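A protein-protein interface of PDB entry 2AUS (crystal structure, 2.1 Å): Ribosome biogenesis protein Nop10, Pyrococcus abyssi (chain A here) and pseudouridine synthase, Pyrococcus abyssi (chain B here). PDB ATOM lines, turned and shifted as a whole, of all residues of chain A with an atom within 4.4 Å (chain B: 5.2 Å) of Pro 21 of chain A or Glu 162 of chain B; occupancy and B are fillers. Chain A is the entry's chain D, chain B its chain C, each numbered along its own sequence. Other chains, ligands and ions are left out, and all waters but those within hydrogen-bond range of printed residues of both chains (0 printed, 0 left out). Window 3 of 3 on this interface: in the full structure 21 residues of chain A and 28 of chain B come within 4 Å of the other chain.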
ATOM      1  N   ARG A  13      19.274 -14.925  -2.955  1.00  0.00           N
ATOM      2  CA  ARG A  13      20.425 -15.568  -3.577  1.00  0.00           C
ATOM      3  C   ARG A  13      21.298 -14.563  -4.320  1.00  0.00           C
ATOM      4  O   ARG A  13      20.793 -13.694  -5.029  1.00  0.00           O
ATOM      5  CB  ARG A  13      19.937 -16.645  -4.551  1.00  0.00           C
ATOM      6  CG  ARG A  13      20.963 -17.120  -5.572  1.00  0.00           C
ATOM      7  CD  ARG A  13      22.084 -17.920  -4.932  1.00  0.00           C
ATOM      8  NE  ARG A  13      22.972 -18.498  -5.938  1.00  0.00           N
ATOM      9  CZ  ARG A  13      24.020 -19.267  -5.658  1.00  0.00           C
ATOM     10  NH1 ARG A  13      24.319 -19.554  -4.397  1.00  0.00           N
ATOM     11  NH2 ARG A  13      24.771 -19.749  -6.641  1.00  0.00           N
ATOM     12  N   THR A  15      23.929 -13.715  -7.218  1.00  0.00           N
ATOM     13  CA  THR A  15      24.229 -14.258  -8.534  1.00  0.00           C
ATOM     14  C   THR A  15      24.685 -13.140  -9.456  1.00  0.00           C
ATOM     15  O   THR A  15      24.533 -11.966  -9.139  1.00  0.00           O
ATOM     16  CB  THR A  15      22.968 -14.913  -9.149  1.00  0.00           C
ATOM     17  OG1 THR A  15      23.248 -15.354 -10.483  1.00  0.00           O
ATOM     18  CG2 THR A  15      21.817 -13.909  -9.184  1.00  0.00           C
ATOM     19  N   LEU A  16      25.253 -13.512 -10.596  1.00  0.00           N
ATOM     20  CA  LEU A  16      25.697 -12.524 -11.567  1.00  0.00           C
ATOM     21  C   LEU A  16      24.650 -12.466 -12.674  1.00  0.00           C
ATOM     22  O   LEU A  16      24.600 -11.512 -13.450  1.00  0.00           O
ATOM     23  CB  LEU A  16      27.048 -12.927 -12.157  1.00  0.00           C
ATOM     24  CG  LEU A  16      28.227 -13.073 -11.195  1.00  0.00           C
ATOM     25  CD1 LEU A  16      29.441 -13.577 -11.967  1.00  0.00           C
ATOM     26  CD2 LEU A  16      28.526 -11.739 -10.533  1.00  0.00           C
ATOM     27  N   LYS A  17      23.808 -13.497 -12.721  1.00  0.00           N
ATOM     28  CA  LYS A  17      22.764 -13.621 -13.732  1.00  0.00           C
ATOM     29  C   LYS A  17      21.615 -12.640 -13.558  1.00  0.00           C
ATOM     30  O   LYS A  17      21.335 -12.178 -12.450  1.00  0.00           O
ATOM     31  CB  LYS A  17      22.214 -15.048 -13.733  1.00  0.00           C
ATOM     32  CG  LYS A  17      23.273 -16.104 -13.987  1.00  0.00           C
ATOM     33  CD  LYS A  17      22.711 -17.503 -13.828  1.00  0.00           C
ATOM     34  CE  LYS A  17      23.764 -18.552 -14.138  1.00  0.00           C
ATOM     35  NZ  LYS A  17      23.251 -19.942 -13.962  1.00  0.00           N
ATOM     36  N   THR A  19      18.504 -13.393 -14.238  1.00  0.00           N
ATOM     37  CA  THR A  19      17.370 -14.152 -13.739  1.00  0.00           C
ATOM     38  C   THR A  19      17.873 -15.126 -12.686  1.00  0.00           C
ATOM     39  O   THR A  19      18.805 -15.891 -12.936  1.00  0.00           O
ATOM     40  CB  THR A  19      16.696 -14.948 -14.877  1.00  0.00           C
ATOM     41  OG1 THR A  19      16.240 -14.041 -15.890  1.00  0.00           O
ATOM     42  CG2 THR A  19      15.517 -15.752 -14.344  1.00  0.00           C
ATOM     43  N   CYS A  20      17.267 -15.096 -11.506  1.00  0.00           N
ATOM     44  CA  CYS A  20      17.685 -15.994 -10.440  1.00  0.00           C
ATOM     45  C   CYS A  20      17.652 -17.438 -10.925  1.00  0.00           C
ATOM     46  O   CYS A  20      16.657 -17.890 -11.497  1.00  0.00           O
ATOM     47  CB  CYS A  20      16.777 -15.843  -9.224  1.00  0.00           C
ATOM     48  SG  CYS A  20      17.222 -16.959  -7.879  1.00  0.00           S
ATOM     49  N   PRO A  21      18.746 -18.182 -10.705  1.00  0.00           N
ATOM     50  CA  PRO A  21      18.839 -19.583 -11.125  1.00  0.00           C
ATOM     51  C   PRO A  21      17.976 -20.564 -10.324  1.00  0.00           C
ATOM     52  O   PRO A  21      17.467 -21.541 -10.878  1.00  0.00           O
ATOM     53  CB  PRO A  21      20.332 -19.881 -10.994  1.00  0.00           C
ATOM     54  CG  PRO A  21      20.742 -19.010  -9.845  1.00  0.00           C
ATOM     55  CD  PRO A  21      20.030 -17.713 -10.155  1.00  0.00           C
ATOM     56  N   VAL A  22      17.797 -20.300  -9.032  1.00  0.00           N
ATOM     57  CA  VAL A  22      17.010 -21.186  -8.176  1.00  0.00           C
ATOM     58  C   VAL A  22      15.525 -20.846  -8.051  1.00  0.00           C
ATOM     59  O   VAL A  22      14.732 -21.683  -7.622  1.00  0.00           O
ATOM     60  CB  VAL A  22      17.604 -21.247  -6.751  1.00  0.00           C
ATOM     61  CG1 VAL A  22      18.974 -21.907  -6.782  1.00  0.00           C
ATOM     62  CG2 VAL A  22      17.697 -19.848  -6.170  1.00  0.00           C
ATOM     63  N   CYS A  23      15.142 -19.629  -8.423  1.00  0.00           N
ATOM     64  CA  CYS A  23      13.744 -19.225  -8.322  1.00  0.00           C
ATOM     65  C   CYS A  23      13.121 -18.852  -9.664  1.00  0.00           C
ATOM     66  O   CYS A  23      11.967 -19.186  -9.934  1.00  0.00           O
ATOM     67  CB  CYS A  23      13.609 -18.055  -7.341  1.00  0.00           C
ATOM     68  SG  CYS A  23      12.810 -16.571  -8.020  1.00  0.00           S
ATOM     69  N   ILE B 160      32.173 -20.851  -3.361  1.00  0.00           N
ATOM     70  CA  ILE B 160      32.005 -20.330  -4.711  1.00  0.00           C
ATOM     71  C   ILE B 160      30.537 -20.414  -5.102  1.00  0.00           C
ATOM     72  O   ILE B 160      29.951 -21.496  -5.137  1.00  0.00           O
ATOM     73  CB  ILE B 160      32.848 -21.126  -5.722  1.00  0.00           C
ATOM     74  CG1 ILE B 160      34.332 -20.929  -5.410  1.00  0.00           C
ATOM     75  CG2 ILE B 160      32.526 -20.675  -7.142  1.00  0.00           C
ATOM     76  CD1 ILE B 160      35.268 -21.693  -6.311  1.00  0.00           C
ATOM     77  N   LEU B 161      29.943 -19.260  -5.371  1.00  0.00           N
ATOM     78  CA  LEU B 161      28.546 -19.196  -5.757  1.00  0.00           C
ATOM     79  C   LEU B 161      28.419 -19.478  -7.246  1.00  0.00           C
ATOM     80  O   LEU B 161      27.724 -20.408  -7.652  1.00  0.00           O
ATOM     81  CB  LEU B 161      27.966 -17.817  -5.431  1.00  0.00           C
ATOM     82  CG  LEU B 161      27.944 -17.427  -3.944  1.00  0.00           C
ATOM     83  CD1 LEU B 161      27.368 -16.029  -3.794  1.00  0.00           C
ATOM     84  CD2 LEU B 161      27.108 -18.426  -3.150  1.00  0.00           C
ATOM     85  N   GLU B 162      29.106 -18.685  -8.062  1.00  0.00           N
ATOM     86  CA  GLU B 162      29.050 -18.875  -9.504  1.00  0.00           C
ATOM     87  C   GLU B 162      30.381 -18.602 -10.187  1.00  0.00           C
ATOM     88  O   GLU B 162      31.178 -17.785  -9.730  1.00  0.00           O
ATOM     89  CB  GLU B 162      27.987 -17.964 -10.125  1.00  0.00           C
ATOM     90  CG  GLU B 162      26.590 -18.130  -9.556  1.00  0.00           C
ATOM     91  CD  GLU B 162      25.568 -17.283 -10.287  1.00  0.00           C
ATOM     92  OE1 GLU B 162      25.973 -16.285 -10.919  1.00  0.00           O
ATOM     93  OE2 GLU B 162      24.361 -17.606 -10.215  1.00  0.00           O
ATOM     94  N   ILE B 163      30.606 -19.300 -11.294  1.00  0.00           N
ATOM     95  CA  ILE B 163      31.814 -19.121 -12.081  1.00  0.00           C
ATOM     96  C   ILE B 163      31.417 -18.956 -13.540  1.00  0.00           C
ATOM     97  O   ILE B 163      30.821 -19.860 -14.125  1.00  0.00           O
ATOM     98  CB  ILE B 163      32.756 -20.338 -11.993  1.00  0.00           C
ATOM     99  CG1 ILE B 163      33.270 -20.511 -10.563  1.00  0.00           C
ATOM    100  CG2 ILE B 163      33.915 -20.157 -12.969  1.00  0.00           C
ATOM    101  CD1 ILE B 163      34.167 -21.714 -10.378  1.00  0.00           C
ATOM    102  N   ASP B 164      31.728 -17.803 -14.120  1.00  0.00           N
ATOM    103  CA  ASP B 164      31.426 -17.572 -15.526  1.00  0.00           C
ATOM    104  C   ASP B 164      32.703 -17.077 -16.201  1.00  0.00           C
ATOM    105  O   ASP B 164      33.006 -15.881 -16.196  1.00  0.00           O
ATOM    106  CB  ASP B 164      30.312 -16.535 -15.698  1.00  0.00           C
ATOM    107  CG  ASP B 164      29.766 -16.494 -17.133  1.00  0.00           C
ATOM    108  OD1 ASP B 164      30.517 -16.844 -18.075  1.00  0.00           O
ATOM    109  OD2 ASP B 164      28.593 -16.102 -17.323  1.00  0.00           O
ATOM    110  N   ASP B 167      35.028 -14.566 -14.391  1.00  0.00           N
ATOM    111  CA  ASP B 167      34.346 -13.994 -13.241  1.00  0.00           C
ATOM    112  C   ASP B 167      33.968 -15.046 -12.215  1.00  0.00           C
ATOM    113  O   ASP B 167      33.325 -16.051 -12.529  1.00  0.00           O
ATOM    114  CB  ASP B 167      33.106 -13.225 -13.695  1.00  0.00           C
ATOM    115  CG  ASP B 167      33.455 -11.987 -14.509  1.00  0.00           C
ATOM    116  OD1 ASP B 167      34.132 -11.084 -13.965  1.00  0.00           O
ATOM    117  OD2 ASP B 167      33.053 -11.922 -15.692  1.00  0.00           O
ATOM    118  N   VAL B 168      34.387 -14.805 -10.980  1.00  0.00           N
ATOM    119  CA  VAL B 168      34.116 -15.731  -9.895  1.00  0.00           C
ATOM    120  C   VAL B 168      33.408 -15.003  -8.770  1.00  0.00           C
ATOM    121  O   VAL B 168      33.951 -14.075  -8.182  1.00  0.00           O
ATOM    122  CB  VAL B 168      35.428 -16.354  -9.353  1.00  0.00           C
ATOM    123  CG1 VAL B 168      35.117 -17.373  -8.253  1.00  0.00           C
ATOM    124  CG2 VAL B 168      36.191 -17.016 -10.489  1.00  0.00           C
ATOM    125  N   LEU B 169      32.179 -15.423  -8.498  1.00  0.00           N
ATOM    126  CA  LEU B 169      31.377 -14.838  -7.434  1.00  0.00           C
ATOM    127  C   LEU B 169      31.465 -15.803  -6.250  1.00  0.00           C
ATOM    128  O   LEU B 169      31.050 -16.961  -6.352  1.00  0.00           O
ATOM    129  CB  LEU B 169      29.921 -14.689  -7.894  1.00  0.00           C
ATOM    130  CG  LEU B 169      28.907 -14.195  -6.857  1.00  0.00           C
ATOM    131  CD1 LEU B 169      29.196 -12.747  -6.486  1.00  0.00           C
ATOM    132  CD2 LEU B 169      27.491 -14.322  -7.423  1.00  0.00           C
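The side-chain hydroxyl (OG1) of Thr 15 of chain A lies within hydrogen-bond range of the side-chain carboxylate (OE2) of Glu 162 of chain B, 2.5 Å away.
NH2 of Arg 13 of chain A sits at hydrogen-bond distance from O of Leu 161 of chain B.
OE1 of Glu 162 of chain B lies within hydrogen-bond range of N of Leu 16 of chain A (2.9 Å).
The backbone carbonyl oxygen (O) of Glu 162 of chain B is in hydrogen-bond range of the backbone NH (N) of Leu 169 of chain B (2.8 Å).
O of Leu 169 of chain B is in hydrogen-bond range of N of Leu 161 of chain B, 2.7 Å away.
N of Lys 17 of chain A lies within hydrogen-bond range of OG1 of Thr 15 of chain A (3.0 Å).
Among the printed residues, merely in contact across the chains: Arg 13 of chain A with Glu 162 of chain B, Thr 15 of chain A with Leu 169 of chain B, Leu 16 of chain A with Leu 169 of chain B, Lys 17 of chain A with Glu 162 of chain B and Pro 21 of chain A with Glu 162 of chain B.
Of the printed residues of chain B, Leu 16 of chain A touches Glu 162 and Leu 169.
Of the printed residues of chain B, Lys 17 of chain A touches Glu 162 (3.96 Å).
Pro 21 of chain A touches just one residue of chain B: Glu 162.
Ile 160 of chain B touches none of the printed residues of chain A.
Of the printed residues of chain A, Leu 161 of chain B touches Arg 13.
Glu 162 of chain B touches just these residues of chain A: Arg 13, Thr 15, Leu 16, Lys 17 and Pro 21.
Of the printed residues of chain A, Leu 169 of chain B touches Thr 15 (3.4 Å) and Leu 16 (3.97 Å).
The nearest printed residue of chain A that does not touch Glu 162 of chain B is Thr 19 of chain A (6.4 Å).
Hydrophobic or aromatic side chains of chain B that line the printed part of chain A: Leu 161 and Leu 169.
Of the 9 printed residues of chain A, 5 touch a printed residue of chain B.
Along chain A the printed residues that touch a printed residue of chain B span positions 13 to 21.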
